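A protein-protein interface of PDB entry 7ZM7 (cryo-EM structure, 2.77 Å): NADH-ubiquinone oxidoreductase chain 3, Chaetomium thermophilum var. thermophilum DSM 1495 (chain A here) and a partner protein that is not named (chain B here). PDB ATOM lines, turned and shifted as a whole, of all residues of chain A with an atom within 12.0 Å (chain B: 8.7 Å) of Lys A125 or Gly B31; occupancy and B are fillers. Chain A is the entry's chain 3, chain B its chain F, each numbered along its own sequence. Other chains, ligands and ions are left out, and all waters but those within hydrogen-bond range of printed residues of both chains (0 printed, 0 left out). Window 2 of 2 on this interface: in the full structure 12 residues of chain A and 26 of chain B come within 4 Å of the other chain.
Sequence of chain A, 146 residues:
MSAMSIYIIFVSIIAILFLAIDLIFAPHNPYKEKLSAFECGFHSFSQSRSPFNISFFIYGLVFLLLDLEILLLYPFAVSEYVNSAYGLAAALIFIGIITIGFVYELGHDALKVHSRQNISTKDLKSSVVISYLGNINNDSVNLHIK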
ATOM      1  N   LEU A 124      -8.213  30.147  24.533  1.00  0.00           N
ATOM      2  CA  LEU A 124      -7.054  30.750  25.180  1.00  0.00           C
ATOM      3  C   LEU A 124      -5.859  29.809  25.132  1.00  0.00           C
ATOM      4  O   LEU A 124      -5.987  28.621  25.427  1.00  0.00           O
ATOM      5  CB  LEU A 124      -7.379  31.121  26.627  1.00  0.00           C
ATOM      6  N   LYS A 125      -4.700  30.351  24.763  1.00  0.00           N
ATOM      7  CA  LYS A 125      -3.492  29.545  24.651  1.00  0.00           C
ATOM      8  C   LYS A 125      -3.125  28.944  26.002  1.00  0.00           C
ATOM      9  O   LYS A 125      -3.289  29.576  27.049  1.00  0.00           O
ATOM     10  CB  LYS A 125      -2.339  30.392  24.116  1.00  0.00           C
ATOM     11  N   SER A 126      -2.631  27.711  25.973  1.00  0.00           N
ATOM     12  CA  SER A 126      -2.303  26.966  27.180  1.00  0.00           C
ATOM     13  C   SER A 126      -0.838  27.167  27.533  1.00  0.00           C
ATOM     14  O   SER A 126       0.025  27.143  26.653  1.00  0.00           O
ATOM     15  CB  SER A 126      -2.602  25.477  26.998  1.00  0.00           C
ATOM     16  OG  SER A 126      -2.125  24.723  28.101  1.00  0.00           O
ATOM     17  N   SER A 127      -0.564  27.351  28.826  1.00  0.00           N
ATOM     18  CA  SER A 127       0.809  27.560  29.272  1.00  0.00           C
ATOM     19  C   SER A 127       1.593  26.258  29.303  1.00  0.00           C
ATOM     20  O   SER A 127       2.826  26.272  29.322  1.00  0.00           O
ATOM     21  CB  SER A 127       0.812  28.212  30.649  1.00  0.00           C
ATOM     22  OG  SER A 127      -0.115  29.279  30.704  1.00  0.00           O
ATOM     23  N   VAL A 128       0.904  25.122  29.312  1.00  0.00           N
ATOM     24  CA  VAL A 128       1.563  23.829  29.464  1.00  0.00           C
ATOM     25  C   VAL A 128       2.145  23.422  28.114  1.00  0.00           C
ATOM     26  O   VAL A 128       1.401  23.180  27.160  1.00  0.00           O
ATOM     27  CB  VAL A 128       0.593  22.769  29.994  1.00  0.00           C
ATOM     28  CG1 VAL A 128       1.288  21.427  30.117  1.00  0.00           C
ATOM     29  CG2 VAL A 128       0.015  23.201  31.316  1.00  0.00           C
ATOM     30  N   VAL A 129       3.468  23.343  28.026  1.00  0.00           N
ATOM     31  CA  VAL A 129       4.169  23.033  26.787  1.00  0.00           C
ATOM     32  C   VAL A 129       5.075  21.839  27.036  1.00  0.00           C
ATOM     33  O   VAL A 129       5.929  21.880  27.926  1.00  0.00           O
ATOM     34  CB  VAL A 129       4.986  24.225  26.280  1.00  0.00           C
ATOM     35  CG1 VAL A 129       5.771  23.830  25.051  1.00  0.00           C
ATOM     36  CG2 VAL A 129       4.090  25.381  25.992  1.00  0.00           C
ATOM     37  N   ILE A 130       4.902  20.787  26.250  1.00  0.00           N
ATOM     38  CA  ILE A 130       5.647  19.553  26.449  1.00  0.00           C
ATOM     39  C   ILE A 130       6.722  19.430  25.388  1.00  0.00           C
ATOM     40  O   ILE A 130       6.560  19.848  24.241  1.00  0.00           O
ATOM     41  CB  ILE A 130       4.741  18.309  26.455  1.00  0.00           C
ATOM     42  CG1 ILE A 130       3.475  18.575  27.246  1.00  0.00           C
ATOM     43  CG2 ILE A 130       5.454  17.143  27.093  1.00  0.00           C
ATOM     44  CD1 ILE A 130       2.407  17.564  26.986  1.00  0.00           C
ATOM     45  N   LEU B  28       1.689  27.510  13.046  1.00  0.00           N
ATOM     46  CA  LEU B  28       0.389  27.838  13.600  1.00  0.00           C
ATOM     47  C   LEU B  28       0.544  28.678  14.854  1.00  0.00           C
ATOM     48  O   LEU B  28       1.298  28.332  15.764  1.00  0.00           O
ATOM     49  CB  LEU B  28      -0.399  26.569  13.911  1.00  0.00           C
ATOM     50  CG  LEU B  28      -0.665  25.681  12.703  1.00  0.00           C
ATOM     51  CD1 LEU B  28      -0.923  24.232  13.114  1.00  0.00           C
ATOM     52  CD2 LEU B  28      -1.804  26.232  11.885  1.00  0.00           C
ATOM     53  N   VAL B  29      -0.190  29.774  14.900  1.00  0.00           N
ATOM     54  CA  VAL B  29      -0.266  30.610  16.096  1.00  0.00           C
ATOM     55  C   VAL B  29      -0.877  29.790  17.226  1.00  0.00           C
ATOM     56  O   VAL B  29      -1.921  29.152  17.020  1.00  0.00           O
ATOM     57  CB  VAL B  29      -1.107  31.851  15.806  1.00  0.00           C
ATOM     58  CG1 VAL B  29      -1.164  32.771  17.020  1.00  0.00           C
ATOM     59  CG2 VAL B  29      -0.590  32.562  14.567  1.00  0.00           C
ATOM     60  N   PRO B  30      -0.263  29.736  18.405  1.00  0.00           N
ATOM     61  CA  PRO B  30      -0.854  28.959  19.496  1.00  0.00           C
ATOM     62  C   PRO B  30      -2.068  29.664  20.069  1.00  0.00           C
ATOM     63  O   PRO B  30      -2.063  30.876  20.281  1.00  0.00           O
ATOM     64  CB  PRO B  30       0.281  28.857  20.524  1.00  0.00           C
ATOM     65  CG  PRO B  30       1.494  29.234  19.811  1.00  0.00           C
ATOM     66  CD  PRO B  30       1.080  30.210  18.753  1.00  0.00           C
ATOM     67  N   GLY B  31      -3.124  28.897  20.290  1.00  0.00           N
ATOM     68  CA  GLY B  31      -4.339  29.451  20.827  1.00  0.00           C
ATOM     69  C   GLY B  31      -5.207  30.166  19.829  1.00  0.00           C
ATOM     70  O   GLY B  31      -6.247  30.698  20.219  1.00  0.00           O
ATOM     71  N   ALA B  32      -4.811  30.210  18.562  1.00  0.00           N
ATOM     72  CA  ALA B  32      -5.695  30.711  17.531  1.00  0.00           C
ATOM     73  C   ALA B  32      -6.890  29.777  17.397  1.00  0.00           C
ATOM     74  O   ALA B  32      -6.772  28.573  17.624  1.00  0.00           O
ATOM     75  CB  ALA B  32      -4.969  30.822  16.199  1.00  0.00           C
ATOM     76  N   PRO B  33      -8.062  30.311  17.085  1.00  0.00           N
ATOM     77  CA  PRO B  33      -9.238  29.451  16.960  1.00  0.00           C
ATOM     78  C   PRO B  33      -9.067  28.439  15.840  1.00  0.00           C
ATOM     79  O   PRO B  33      -8.504  28.731  14.786  1.00  0.00           O
ATOM     80  CB  PRO B  33     -10.368  30.443  16.672  1.00  0.00           C
ATOM     81  CG  PRO B  33      -9.705  31.625  16.139  1.00  0.00           C
ATOM     82  CD  PRO B  33      -8.393  31.722  16.848  1.00  0.00           C
ATOM     83  N   THR B  34      -9.568  27.238  16.076  1.00  0.00           N
ATOM     84  CA  THR B  34      -9.421  26.155  15.125  1.00  0.00           C
ATOM     85  C   THR B  34     -10.584  26.043  14.153  1.00  0.00           C
ATOM     86  O   THR B  34     -10.450  25.375  13.128  1.00  0.00           O
ATOM     87  CB  THR B  34      -9.255  24.826  15.873  1.00  0.00           C
ATOM     88  OG1 THR B  34     -10.344  24.644  16.786  1.00  0.00           O
ATOM     89  CG2 THR B  34      -7.961  24.808  16.655  1.00  0.00           C
ATOM     90  N   GLY B  38     -14.101  26.883  21.393  1.00  0.00           N
ATOM     91  CA  GLY B  38     -13.512  26.430  22.625  1.00  0.00           C
ATOM     92  C   GLY B  38     -12.256  25.611  22.472  1.00  0.00           C
ATOM     93  O   GLY B  38     -11.614  25.301  23.476  1.00  0.00           O
ATOM     94  N   LEU B  39     -11.882  25.256  21.256  1.00  0.00           N
ATOM     95  CA  LEU B  39     -10.694  24.459  21.000  1.00  0.00           C
ATOM     96  C   LEU B  39      -9.680  25.340  20.287  1.00  0.00           C
ATOM     97  O   LEU B  39      -9.918  25.782  19.162  1.00  0.00           O
ATOM     98  CB  LEU B  39     -11.040  23.217  20.178  1.00  0.00           C
ATOM     99  CG  LEU B  39      -9.904  22.215  19.976  1.00  0.00           C
ATOM    100  CD1 LEU B  39      -9.745  21.274  21.147  1.00  0.00           C
ATOM    101  CD2 LEU B  39     -10.102  21.450  18.693  1.00  0.00           C
ATOM    102  N   GLY B  40      -8.565  25.608  20.947  1.00  0.00           N
ATOM    103  CA  GLY B  40      -7.564  26.494  20.400  1.00  0.00           C
ATOM    104  C   GLY B  40      -6.281  25.775  20.057  1.00  0.00           C
ATOM    105  O   GLY B  40      -6.000  24.709  20.608  1.00  0.00           O
ATOM    106  N   THR B  41      -5.498  26.354  19.154  1.00  0.00           N
ATOM    107  CA  THR B  41      -4.351  25.665  18.578  1.00  0.00           C
ATOM    108  C   THR B  41      -3.337  25.277  19.648  1.00  0.00           C
ATOM    109  O   THR B  41      -2.990  26.077  20.518  1.00  0.00           O
ATOM    110  CB  THR B  41      -3.705  26.548  17.531  1.00  0.00           C
ATOM    111  OG1 THR B  41      -4.575  26.661  16.402  1.00  0.00           O
ATOM    112  CG2 THR B  41      -2.400  25.954  17.084  1.00  0.00           C
ATOM    113  N   HIS B  42      -2.912  24.013  19.648  1.00  0.00           N
ATOM    114  CA  HIS B  42      -1.987  23.518  20.708  1.00  0.00           C
ATOM    115  C   HIS B  42      -0.607  24.169  20.577  1.00  0.00           C
ATOM    116  O   HIS B  42      -0.084  24.235  19.457  1.00  0.00           O
ATOM    117  CB  HIS B  42      -1.889  21.987  20.678  1.00  0.00           C
ATOM    118  CG  HIS B  42      -1.636  21.376  22.014  1.00  0.00           C
ATOM    119  ND1 HIS B  42      -2.661  20.986  22.851  1.00  0.00           N
ATOM    120  CD2 HIS B  42      -0.488  21.089  22.662  1.00  0.00           C
ATOM    121  CE1 HIS B  42      -2.157  20.481  23.957  1.00  0.00           C
ATOM    122  NE2 HIS B  42      -0.825  20.536  23.868  1.00  0.00           N
ATOM    123  N   PRO B  43       0.010  24.630  21.682  1.00  0.00           N
ATOM    124  CA  PRO B  43       1.348  25.210  21.623  1.00  0.00           C
ATOM    125  C   PRO B  43       2.405  24.209  21.131  1.00  0.00           C
ATOM    126  O   PRO B  43       3.230  24.619  20.350  1.00  0.00           O
ATOM    127  CB  PRO B  43       1.597  25.676  23.064  1.00  0.00           C
ATOM    128  CG  PRO B  43       0.666  24.832  23.903  1.00  0.00           C
ATOM    129  CD  PRO B  43      -0.556  24.641  23.032  1.00  0.00           C
ATOM    130  N   SER B  44       2.355  22.951  21.574  1.00  0.00           N
ATOM    131  CA  SER B  44       3.287  21.898  21.090  1.00  0.00           C
ATOM    132  C   SER B  44       2.461  20.648  20.773  1.00  0.00           C
ATOM    133  O   SER B  44       2.387  19.783  21.659  1.00  0.00           O
ATOM    134  CB  SER B  44       4.327  21.598  22.137  1.00  0.00           C
ATOM    135  OG  SER B  44       3.726  21.348  23.399  1.00  0.00           O
ATOM    136  N   LEU B 143       4.759  28.261  31.021  1.00  0.00           N
ATOM    137  CA  LEU B 143       5.313  29.563  30.708  1.00  0.00           C
ATOM    138  C   LEU B 143       4.447  30.659  31.310  1.00  0.00           C
ATOM    139  O   LEU B 143       3.216  30.557  31.284  1.00  0.00           O
ATOM    140  CB  LEU B 143       5.394  29.737  29.192  1.00  0.00           C
ATOM    141  CG  LEU B 143       6.007  30.996  28.593  1.00  0.00           C
ATOM    142  CD1 LEU B 143       7.464  31.094  28.986  1.00  0.00           C
ATOM    143  CD2 LEU B 143       5.865  30.975  27.083  1.00  0.00           C
ATOM    144  N   LYS B 145       2.144  33.757  31.684  1.00  0.00           N
ATOM    145  CA  LYS B 145       1.196  34.262  30.702  1.00  0.00           C
ATOM    146  C   LYS B 145       1.616  35.636  30.200  1.00  0.00           C
ATOM    147  O   LYS B 145       2.041  36.496  30.976  1.00  0.00           O
ATOM    148  CB  LYS B 145      -0.202  34.330  31.310  1.00  0.00           C
ATOM    149  CG  LYS B 145      -0.689  33.007  31.873  1.00  0.00           C
ATOM    150  CD  LYS B 145      -2.015  33.167  32.594  1.00  0.00           C
ATOM    151  CE  LYS B 145      -1.876  34.076  33.801  1.00  0.00           C
ATOM    152  NZ  LYS B 145      -0.857  33.562  34.757  1.00  0.00           N
ATOM    153  N   GLU B 146       1.495  35.842  28.891  1.00  0.00           N
ATOM    154  CA  GLU B 146       1.821  37.122  28.274  1.00  0.00           C
ATOM    155  C   GLU B 146       0.643  38.064  28.480  1.00  0.00           C
ATOM    156  O   GLU B 146      -0.442  37.839  27.937  1.00  0.00           O
ATOM    157  CB  GLU B 146       2.125  36.959  26.788  1.00  0.00           C
ATOM    158  CG  GLU B 146       3.249  35.998  26.475  1.00  0.00           C
ATOM    159  CD  GLU B 146       2.762  34.571  26.361  1.00  0.00           C
ATOM    160  OE1 GLU B 146       1.540  34.377  26.203  1.00  0.00           O
ATOM    161  OE2 GLU B 146       3.600  33.648  26.423  1.00  0.00           O
ATOM    162  N   GLU B 147       0.856  39.117  29.258  1.00  0.00           N
ATOM    163  CA  GLU B 147      -0.175  40.102  29.529  1.00  0.00           C
ATOM    164  C   GLU B 147       0.312  41.482  29.117  1.00  0.00           C
ATOM    165  O   GLU B 147       1.512  41.720  28.957  1.00  0.00           O
ATOM    166  CB  GLU B 147      -0.570  40.105  31.008  1.00  0.00           C
ATOM    167  CG  GLU B 147      -0.932  38.737  31.539  1.00  0.00           C
ATOM    168  CD  GLU B 147      -1.979  38.051  30.690  1.00  0.00           C
ATOM    169  OE1 GLU B 147      -3.037  38.665  30.440  1.00  0.00           O
ATOM    170  OE2 GLU B 147      -1.743  36.900  30.269  1.00  0.00           O
ATOM    171  N   GLU B 220      -5.465  19.146  17.338  1.00  0.00           N
ATOM    172  CA  GLU B 220      -5.918  19.505  18.670  1.00  0.00           C
ATOM    173  C   GLU B 220      -7.083  18.633  19.105  1.00  0.00           C
ATOM    174  O   GLU B 220      -7.263  18.367  20.296  1.00  0.00           O
ATOM    175  CB  GLU B 220      -6.283  20.984  18.700  1.00  0.00           C
ATOM    176  CG  GLU B 220      -5.129  21.893  18.338  1.00  0.00           C
ATOM    177  CD  GLU B 220      -5.069  22.239  16.862  1.00  0.00           C
ATOM    178  OE1 GLU B 220      -5.825  21.650  16.069  1.00  0.00           O
ATOM    179  OE2 GLU B 220      -4.258  23.104  16.491  1.00  0.00           O
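Of the 19 printed residues of chain B, 6 touch a printed residue of chain A. Among the printed residues, 9 pairs touch across the chains. Among the printed residues, no Asp or Glu carboxylate lies within 4 Å of a Lys or Arg side-chain nitrogen of the other chain.
Among the printed residues, pairs that only touch across the chains: Lys A125 with Pro B30 (3.9 Å), Lys A125 with Gly B31 (3.9 Å), Ser A126 with Pro B43 (3.6 Å), Ser A127 with Lys B145 (3.9 Å), Val A128 with Pro B43 (3.7 Å), Val A129 with Pro B43 (3.9 Å) and Val A129 with Ser B44 (3.6 Å).
O of Thr B41 is in hydrogen-bond range of N of Gly B31, at 2.8 Å. The backbone NH (N) of Val A128 sits close to the side-chain hydroxyl (OG) of Ser A126.
The side-chain hydroxyl (OG) of Ser B44 lies within hydrogen-bond range of the backbone NH (N) of Ile A130 (3.1 Å). The backbone NH (N) of Leu B143 lies within hydrogen-bond range of the backbone carbonyl oxygen (O) of Ser A127, 3.3 Å away.
No residue of chain B comes within 4 Å of Leu A124. Of chain B, only Pro B30 (3.9 Å) and Gly B31 (3.9 Å) come within 4 Å of Lys A125. Of the printed residues of chain B, Ser A126 touches Pro B43 (3.6 Å). Of the printed residues of chain B, Ser A127 touches Leu B143 and Lys B145. Of the printed residues of chain B, Val A128 touches Pro B43. Val B29 touches none of the printed residues of chain A. Of chain A, only Lys A125 (3.9 Å) comes within 4 Å of Gly B31. Pro B33 touches none of the printed residues of chain A. Thr B34 touches none of the printed residues of chain A. No residue of chain A comes within 4 Å of Gly B40. No residue of chain A comes within 4 Å of Thr B41. His B42 touches none of the printed residues of chain A. Pro B43 touches just these residues of chain A: Ser A126, Val A128 and Val A129. Printed residues of chain A within 4 Å of Ser B44: Val A129 and Ile A130. Of the printed residues of chain A, Lys B145 touches Ser A127. The nearest residue of chain B that does not touch Lys A125 is Thr B41 (5.4 Å). The nearest residue of chain A that does not touch Gly B31 is Leu A124 (4.6 Å).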
